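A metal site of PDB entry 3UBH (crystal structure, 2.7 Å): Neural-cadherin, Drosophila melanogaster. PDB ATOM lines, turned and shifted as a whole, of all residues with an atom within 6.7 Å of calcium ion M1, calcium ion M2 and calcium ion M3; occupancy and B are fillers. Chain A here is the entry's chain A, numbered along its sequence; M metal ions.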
ATOM      1  N   GLU A  18      22.853 -21.646  21.655  1.00  0.00           N
ATOM      2  CA  GLU A  18      23.037 -22.859  22.424  1.00  0.00           C
ATOM      3  C   GLU A  18      24.491 -23.099  22.778  1.00  0.00           C
ATOM      4  O   GLU A  18      24.840 -23.213  23.950  1.00  0.00           O
ATOM      5  CB  GLU A  18      22.576 -24.006  21.534  1.00  0.00           C
ATOM      6  CG  GLU A  18      21.848 -25.109  22.203  1.00  0.00           C
ATOM      7  CD  GLU A  18      21.267 -26.059  21.193  1.00  0.00           C
ATOM      8  OE1 GLU A  18      21.297 -25.729  19.990  1.00  0.00           O
ATOM      9  OE2 GLU A  18      20.792 -27.136  21.599  1.00  0.00           O
ATOM     10  N   TRP A  63      23.356 -25.617  27.947  1.00  0.00           N
ATOM     11  CA  TRP A  63      22.222 -25.030  27.249  1.00  0.00           C
ATOM     12  C   TRP A  63      21.789 -25.888  26.062  1.00  0.00           C
ATOM     13  O   TRP A  63      22.615 -26.483  25.359  1.00  0.00           O
ATOM     14  CB  TRP A  63      22.561 -23.620  26.791  1.00  0.00           C
ATOM     15  CG  TRP A  63      22.698 -22.632  27.913  1.00  0.00           C
ATOM     16  CD1 TRP A  63      22.614 -22.882  29.266  1.00  0.00           C
ATOM     17  CD2 TRP A  63      22.980 -21.240  27.795  1.00  0.00           C
ATOM     18  NE1 TRP A  63      22.810 -21.722  29.976  1.00  0.00           N
ATOM     19  CE2 TRP A  63      23.032 -20.706  29.094  1.00  0.00           C
ATOM     20  CE3 TRP A  63      23.181 -20.384  26.693  1.00  0.00           C
ATOM     21  CZ2 TRP A  63      23.276 -19.360  29.340  1.00  0.00           C
ATOM     22  CZ3 TRP A  63      23.425 -19.039  26.940  1.00  0.00           C
ATOM     23  CH2 TRP A  63      23.488 -18.543  28.258  1.00  0.00           C
ATOM     24  N   ASP A  64      20.484 -25.967  25.877  1.00  0.00           N
ATOM     25  CA  ASP A  64      19.939 -26.898  24.908  1.00  0.00           C
ATOM     26  C   ASP A  64      18.664 -26.346  24.299  1.00  0.00           C
ATOM     27  O   ASP A  64      17.628 -26.290  24.960  1.00  0.00           O
ATOM     28  CB  ASP A  64      19.667 -28.231  25.589  1.00  0.00           C
ATOM     29  CG  ASP A  64      19.606 -29.375  24.608  1.00  0.00           C
ATOM     30  OD1 ASP A  64      19.363 -29.151  23.404  1.00  0.00           O
ATOM     31  OD2 ASP A  64      19.821 -30.516  25.058  1.00  0.00           O
ATOM     32  N   TYR A  65      18.757 -25.938  23.043  1.00  0.00           N
ATOM     33  CA  TYR A  65      17.622 -25.461  22.279  1.00  0.00           C
ATOM     34  C   TYR A  65      16.558 -26.528  22.194  1.00  0.00           C
ATOM     35  O   TYR A  65      15.377 -26.237  22.317  1.00  0.00           O
ATOM     36  CB  TYR A  65      18.070 -25.045  20.878  1.00  0.00           C
ATOM     37  CG  TYR A  65      17.006 -24.370  20.030  1.00  0.00           C
ATOM     38  CD1 TYR A  65      16.808 -22.996  20.106  1.00  0.00           C
ATOM     39  CD2 TYR A  65      16.224 -25.103  19.144  1.00  0.00           C
ATOM     40  CE1 TYR A  65      15.846 -22.356  19.328  1.00  0.00           C
ATOM     41  CE2 TYR A  65      15.244 -24.482  18.356  1.00  0.00           C
ATOM     42  CZ  TYR A  65      15.064 -23.097  18.457  1.00  0.00           C
ATOM     43  OH  TYR A  65      14.116 -22.466  17.694  1.00  0.00           O
ATOM     44  N   GLU A  66      16.978 -27.776  22.001  1.00  0.00           N
ATOM     45  CA  GLU A  66      16.070 -28.920  21.862  1.00  0.00           C
ATOM     46  C   GLU A  66      15.252 -29.230  23.130  1.00  0.00           C
ATOM     47  O   GLU A  66      14.300 -29.988  23.078  1.00  0.00           O
ATOM     48  CB  GLU A  66      16.856 -30.168  21.435  1.00  0.00           C
ATOM     49  CG  GLU A  66      17.291 -30.202  19.980  1.00  0.00           C
ATOM     50  CD  GLU A  66      18.309 -29.118  19.605  1.00  0.00           C
ATOM     51  OE1 GLU A  66      19.380 -29.006  20.236  1.00  0.00           O
ATOM     52  OE2 GLU A  66      18.026 -28.374  18.645  1.00  0.00           O
ATOM     53  N   GLU A  67      15.628 -28.638  24.263  1.00  0.00           N
ATOM     54  CA  GLU A  67      14.972 -28.972  25.529  1.00  0.00           C
ATOM     55  C   GLU A  67      14.239 -27.778  26.159  1.00  0.00           C
ATOM     56  O   GLU A  67      13.597 -27.912  27.188  1.00  0.00           O
ATOM     57  CB  GLU A  67      15.963 -29.592  26.509  1.00  0.00           C
ATOM     58  CG  GLU A  67      15.470 -30.894  27.165  1.00  0.00           C
ATOM     59  CD  GLU A  67      15.597 -30.890  28.691  1.00  0.00           C
ATOM     60  OE1 GLU A  67      16.563 -30.293  29.228  1.00  0.00           O
ATOM     61  OE2 GLU A  67      14.703 -31.490  29.347  1.00  0.00           O
ATOM     62  N   LYS A 102      19.480 -19.216  20.574  1.00  0.00           N
ATOM     63  CA  LYS A 102      19.397 -19.586  19.158  1.00  0.00           C
ATOM     64  C   LYS A 102      19.847 -21.022  18.877  1.00  0.00           C
ATOM     65  O   LYS A 102      20.771 -21.541  19.516  1.00  0.00           O
ATOM     66  CB  LYS A 102      20.139 -18.562  18.288  1.00  0.00           C
ATOM     67  CG  LYS A 102      19.412 -17.212  18.190  1.00  0.00           C
ATOM     68  CD  LYS A 102      18.212 -17.268  17.241  1.00  0.00           C
ATOM     69  CE  LYS A 102      17.039 -16.436  17.773  1.00  0.00           C
ATOM     70  NZ  LYS A 102      16.029 -16.091  16.702  1.00  0.00           N
ATOM     71  N   ASP A 103      19.175 -21.654  17.930  1.00  0.00           N
ATOM     72  CA  ASP A 103      19.459 -23.044  17.573  1.00  0.00           C
ATOM     73  C   ASP A 103      20.823 -23.222  16.922  1.00  0.00           C
ATOM     74  O   ASP A 103      21.281 -22.384  16.154  1.00  0.00           O
ATOM     75  CB  ASP A 103      18.362 -23.601  16.646  1.00  0.00           C
ATOM     76  CG  ASP A 103      18.392 -25.122  16.539  1.00  0.00           C
ATOM     77  OD1 ASP A 103      18.923 -25.804  17.447  1.00  0.00           O
ATOM     78  OD2 ASP A 103      17.880 -25.647  15.531  1.00  0.00           O
ATOM     79  N   VAL A 104      21.473 -24.319  17.275  1.00  0.00           N
ATOM     80  CA  VAL A 104      22.664 -24.778  16.586  1.00  0.00           C
ATOM     81  C   VAL A 104      22.416 -26.243  16.255  1.00  0.00           C
ATOM     82  O   VAL A 104      21.889 -26.994  17.081  1.00  0.00           O
ATOM     83  CB  VAL A 104      23.955 -24.639  17.464  1.00  0.00           C
ATOM     84  CG1 VAL A 104      25.180 -25.181  16.734  1.00  0.00           C
ATOM     85  CG2 VAL A 104      24.183 -23.204  17.871  1.00  0.00           C
ATOM     86  N   ASN A 105      22.793 -26.641  15.040  1.00  0.00           N
ATOM     87  CA  ASN A 105      22.764 -28.045  14.651  1.00  0.00           C
ATOM     88  C   ASN A 105      23.790 -28.856  15.453  1.00  0.00           C
ATOM     89  O   ASN A 105      24.914 -29.077  14.992  1.00  0.00           O
ATOM     90  CB  ASN A 105      23.011 -28.163  13.158  1.00  0.00           C
ATOM     91  CG  ASN A 105      22.681 -29.528  12.627  1.00  0.00           C
ATOM     92  OD1 ASN A 105      22.898 -30.541  13.295  1.00  0.00           O
ATOM     93  ND2 ASN A 105      22.152 -29.580  11.402  1.00  0.00           N
ATOM     94  N   ASP A 106      23.393 -29.326  16.633  1.00  0.00           N
ATOM     95  CA  ASP A 106      24.348 -29.886  17.599  1.00  0.00           C
ATOM     96  C   ASP A 106      24.014 -31.307  18.051  1.00  0.00           C
ATOM     97  O   ASP A 106      24.719 -31.886  18.897  1.00  0.00           O
ATOM     98  CB  ASP A 106      24.442 -28.967  18.822  1.00  0.00           C
ATOM     99  CG  ASP A 106      23.155 -28.908  19.638  1.00  0.00           C
ATOM    100  OD1 ASP A 106      22.040 -28.913  19.061  1.00  0.00           O
ATOM    101  OD2 ASP A 106      23.249 -28.849  20.876  1.00  0.00           O
ATOM    102  N   GLU A 107      22.929 -31.865  17.489  1.00  0.00           N
ATOM    103  CA  GLU A 107      22.488 -33.212  17.839  1.00  0.00           C
ATOM    104  C   GLU A 107      22.520 -34.103  16.614  1.00  0.00           C
ATOM    105  O   GLU A 107      22.040 -33.716  15.546  1.00  0.00           O
ATOM    106  CB  GLU A 107      21.067 -33.174  18.403  1.00  0.00           C
ATOM    107  CG  GLU A 107      20.802 -32.099  19.454  1.00  0.00           C
ATOM    108  CD  GLU A 107      21.616 -32.236  20.721  1.00  0.00           C
ATOM    109  OE1 GLU A 107      22.089 -33.337  21.037  1.00  0.00           O
ATOM    110  OE2 GLU A 107      21.783 -31.217  21.420  1.00  0.00           O
ATOM    111  N   PRO A 108      23.098 -35.318  16.756  1.00  0.00           N
ATOM    112  CA  PRO A 108      23.248 -36.249  15.624  1.00  0.00           C
ATOM    113  C   PRO A 108      21.922 -36.888  15.227  1.00  0.00           C
ATOM    114  O   PRO A 108      21.019 -36.967  16.064  1.00  0.00           O
ATOM    115  CB  PRO A 108      24.163 -37.334  16.190  1.00  0.00           C
ATOM    116  CG  PRO A 108      23.885 -37.328  17.679  1.00  0.00           C
ATOM    117  CD  PRO A 108      23.620 -35.885  18.016  1.00  0.00           C
ATOM    118  N   PRO A 109      21.819 -37.355  13.969  1.00  0.00           N
ATOM    119  CA  PRO A 109      20.649 -38.064  13.502  1.00  0.00           C
ATOM    120  C   PRO A 109      20.632 -39.493  14.066  1.00  0.00           C
ATOM    121  O   PRO A 109      21.660 -39.955  14.577  1.00  0.00           O
ATOM    122  CB  PRO A 109      20.864 -38.093  11.990  1.00  0.00           C
ATOM    123  CG  PRO A 109      22.293 -38.123  11.822  1.00  0.00           C
ATOM    124  CD  PRO A 109      22.820 -37.237  12.898  1.00  0.00           C
ATOM    125  N   ASP A 139      16.231 -36.329  13.144  1.00  0.00           N
ATOM    126  CA  ASP A 139      17.248 -35.427  13.670  1.00  0.00           C
ATOM    127  C   ASP A 139      16.583 -34.308  14.455  1.00  0.00           C
ATOM    128  O   ASP A 139      15.726 -33.593  13.918  1.00  0.00           O
ATOM    129  CB  ASP A 139      18.114 -34.865  12.545  1.00  0.00           C
ATOM    130  CG  ASP A 139      19.286 -34.026  13.056  1.00  0.00           C
ATOM    131  OD1 ASP A 139      19.055 -32.922  13.592  1.00  0.00           O
ATOM    132  OD2 ASP A 139      20.443 -34.478  12.931  1.00  0.00           O
ATOM    133  N   PRO A 140      16.982 -34.134  15.717  1.00  0.00           N
ATOM    134  CA  PRO A 140      16.337 -33.214  16.629  1.00  0.00           C
ATOM    135  C   PRO A 140      16.423 -31.747  16.217  1.00  0.00           C
ATOM    136  O   PRO A 140      15.595 -30.959  16.668  1.00  0.00           O
ATOM    137  CB  PRO A 140      17.094 -33.436  17.952  1.00  0.00           C
ATOM    138  CG  PRO A 140      17.726 -34.748  17.826  1.00  0.00           C
ATOM    139  CD  PRO A 140      18.088 -34.847  16.372  1.00  0.00           C
ATOM    140  N   ASP A 141      17.420 -31.381  15.405  1.00  0.00           N
ATOM    141  CA  ASP A 141      17.674 -29.981  15.046  1.00  0.00           C
ATOM    142  C   ASP A 141      16.680 -29.450  14.022  1.00  0.00           C
ATOM    143  O   ASP A 141      16.202 -30.200  13.186  1.00  0.00           O
ATOM    144  CB  ASP A 141      19.099 -29.806  14.517  1.00  0.00           C
ATOM    145  CG  ASP A 141      20.147 -29.980  15.581  1.00  0.00           C
ATOM    146  OD1 ASP A 141      20.940 -30.942  15.482  1.00  0.00           O
ATOM    147  OD2 ASP A 141      20.192 -29.169  16.527  1.00  0.00           O
ATOM    148  N   THR A 142      16.398 -28.156  14.087  1.00  0.00           N
ATOM    149  CA  THR A 142      15.365 -27.529  13.259  1.00  0.00           C
ATOM    150  C   THR A 142      15.638 -27.615  11.756  1.00  0.00           C
ATOM    151  O   THR A 142      14.749 -27.960  10.967  1.00  0.00           O
ATOM    152  CB  THR A 142      15.140 -26.053  13.663  1.00  0.00           C
ATOM    153  OG1 THR A 142      16.394 -25.349  13.636  1.00  0.00           O
ATOM    154  CG2 THR A 142      14.530 -25.957  15.069  1.00  0.00           C
ATOM    155  N   ASP A 143      16.885 -27.322  11.365  1.00  0.00           N
ATOM    156  CA  ASP A 143      17.287 -27.268   9.960  1.00  0.00           C
ATOM    157  C   ASP A 143      18.062 -28.501   9.458  1.00  0.00           C
ATOM    158  O   ASP A 143      18.918 -28.377   8.594  1.00  0.00           O
ATOM    159  CB  ASP A 143      18.114 -25.998   9.713  1.00  0.00           C
ATOM    160  CG  ASP A 143      19.551 -26.088  10.276  1.00  0.00           C
ATOM    161  OD1 ASP A 143      20.463 -25.522   9.634  1.00  0.00           O
ATOM    162  OD2 ASP A 143      19.771 -26.701  11.359  1.00  0.00           O
ATOM    163  N   HIS A 144      17.738 -29.690   9.980  1.00  0.00           N
ATOM    164  CA  HIS A 144      18.421 -30.925   9.575  1.00  0.00           C
ATOM    165  C   HIS A 144      18.390 -31.228   8.068  1.00  0.00           C
ATOM    166  O   HIS A 144      17.548 -30.717   7.327  1.00  0.00           O
ATOM    167  CB  HIS A 144      17.875 -32.120  10.343  1.00  0.00           C
ATOM    168  CG  HIS A 144      16.422 -32.386  10.088  1.00  0.00           C
ATOM    169  ND1 HIS A 144      15.957 -32.923   8.906  1.00  0.00           N
ATOM    170  CD2 HIS A 144      15.336 -32.213  10.879  1.00  0.00           C
ATOM    171  CE1 HIS A 144      14.640 -33.052   8.980  1.00  0.00           C
ATOM    172  NE2 HIS A 144      14.242 -32.629  10.162  1.00  0.00           N
ATOM    173  N   ASN A 145      19.313 -32.055   7.621  1.00  0.00           N
ATOM    174  CA  ASN A 145      19.443 -32.346   6.207  1.00  0.00           C
ATOM    175  C   ASN A 145      19.950 -33.765   6.057  1.00  0.00           C
ATOM    176  O   ASN A 145      21.149 -34.001   5.889  1.00  0.00           O
ATOM    177  CB  ASN A 145      20.379 -31.339   5.531  1.00  0.00           C
ATOM    178  CG  ASN A 145      20.446 -31.511   4.028  1.00  0.00           C
ATOM    179  OD1 ASN A 145      19.754 -32.356   3.440  1.00  0.00           O
ATOM    180  ND2 ASN A 145      21.291 -30.711   3.388  1.00  0.00           N
ATOM    181  N   ASP A 190      23.612 -35.896   8.798  1.00  0.00           N
ATOM    182  CA  ASP A 190      22.968 -34.597   8.737  1.00  0.00           C
ATOM    183  C   ASP A 190      24.006 -33.623   8.211  1.00  0.00           C
ATOM    184  O   ASP A 190      24.975 -33.302   8.896  1.00  0.00           O
ATOM    185  CB  ASP A 190      22.464 -34.200  10.135  1.00  0.00           C
ATOM    186  CG  ASP A 190      21.886 -32.805  10.172  1.00  0.00           C
ATOM    187  OD1 ASP A 190      21.645 -32.203   9.109  1.00  0.00           O
ATOM    188  OD2 ASP A 190      21.657 -32.320  11.304  1.00  0.00           O
ATOM    189  N   ASN A 192      23.758 -30.501   7.437  1.00  0.00           N
ATOM    190  CA  ASN A 192      23.696 -29.142   7.923  1.00  0.00           C
ATOM    191  C   ASN A 192      24.477 -28.977   9.217  1.00  0.00           C
ATOM    192  O   ASN A 192      24.673 -27.854   9.683  1.00  0.00           O
ATOM    193  CB  ASN A 192      22.247 -28.681   8.058  1.00  0.00           C
ATOM    194  CG  ASN A 192      21.669 -28.170   6.745  1.00  0.00           C
ATOM    195  OD1 ASN A 192      22.201 -28.419   5.664  1.00  0.00           O
ATOM    196  ND2 ASN A 192      20.560 -27.451   6.833  1.00  0.00           N
ATOM    197  N   GLY A 193      24.936 -30.092   9.784  1.00  0.00           N
ATOM    198  CA  GLY A 193      25.794 -30.076  10.985  1.00  0.00           C
ATOM    199  C   GLY A 193      27.079 -30.908  10.882  1.00  0.00           C
ATOM    200  O   GLY A 193      27.078 -31.988  10.291  1.00  0.00           O
ATOM    201  N   GLN A 201      27.861 -34.834  11.080  1.00  0.00           N
ATOM    202  CA  GLN A 201      27.110 -35.573  12.096  1.00  0.00           C
ATOM    203  C   GLN A 201      26.555 -36.832  11.455  1.00  0.00           C
ATOM    204  O   GLN A 201      26.177 -36.814  10.281  1.00  0.00           O
ATOM    205  CB  GLN A 201      25.923 -34.765  12.597  1.00  0.00           C
ATOM    206  CG  GLN A 201      26.230 -33.624  13.539  1.00  0.00           C
ATOM    207  CD  GLN A 201      24.966 -32.835  13.845  1.00  0.00           C
ATOM    208  OE1 GLN A 201      23.867 -33.225  13.425  1.00  0.00           O
ATOM    209  NE2 GLN A 201      25.109 -31.737  14.551  1.00  0.00           N
HETATM  210 CA    CA M   1      20.184 -27.597  18.197  1.00  0.00          CA
HETATM  211 CA    CA M   2      21.106 -29.136  21.977  1.00  0.00          CA
HETATM  212 CA    CA M   3      21.531 -32.540  13.555  1.00  0.00          CA
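Within 4 Å of calcium ion M3: Asn 105, Glu 107, Asp 139, Asp 141, Asp 190 and Gln 201.
Calcium ion M3 is bound by the side-chain carboxylate (OD2) of Asp 190, the side-chain carboxylate (OD2) of Asp 139, the backbone carbonyl oxygen (O) of Glu 107, the side-chain amide oxygen (OD1) of Asn 105, the side-chain amide oxygen (OE1) of Gln 201, the side-chain carboxylate (OD1) of Asp 139 and the side-chain carboxylate (OD1) of Asp 141.
The backbone carbonyl oxygen (O) of Val 104 binds calcium ion M1 (2.1 Å). The side-chain carboxylate (OD2) of Asp 141 is bound to calcium ion M1, 2.3 Å away. Calcium ion M1 is bound by the side-chain carboxylate (OD1) of Asp 103. Calcium ion M1 is bound by OE2 of Glu 66, at 2.3 Å. OD1 of Asp 106 binds calcium ion M1, at 2.4 Å. The side-chain carboxylate (OE1) of Glu 66 binds calcium ion M1, at 2.6 Å. Calcium ion M1 is bound by OE1 of Glu 18. Calcium ion M1 has seven donor atoms within binding distance.
Calcium ion M2 is bound by OE2 of Glu 18 (2.1 Å), OD1 of Asp 64 (2.3 Å), OE2 of Glu 107 (2.3 Å), OD2 of Asp 106 (2.4 Å) and OE1 of Glu 66 (2.5 Å). Calcium ion M2 has five donor atoms within binding distance. Slightly farther from calcium ion M2 lies OD1 of Asp 106 (3.1 Å).
Six residues have an atom within 4 Å of calcium ion M1: Glu 18, Glu 66, Asp 103, Val 104, Asp 106 and Asp 141.
The side-chain carboxylate of Asp 103 sits at hydrogen-bond distance from the side-chain hydroxyl of Thr 142 (2.4 Å). The backbone NH (N) of Glu 18 sits at hydrogen-bond distance from the backbone carbonyl oxygen (O) of Lys 102, at 3.0 Å. The side-chain amide nitrogen (ND2) of Asn 105 lies close to the backbone NH (N) of Gly 193 (3.3 Å). OD1 of Asp 190 lies within hydrogen-bond range of N of Asn 192, at 3.2 Å. N of Gln 201 lies within hydrogen-bond range of O of Gly 193, 3.1 Å away. N of Asn 145 is in hydrogen-bond range of OD1 of Asp 190 (2.8 Å). The backbone NH (N) of Tyr 65 lies close to the side-chain carboxylate (OE2) of Glu 18, at 2.8 Å.
Five residues have an atom within 4 Å of calcium ion M2: Glu 18, Asp 64, Glu 66, Asp 106 and Glu 107.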
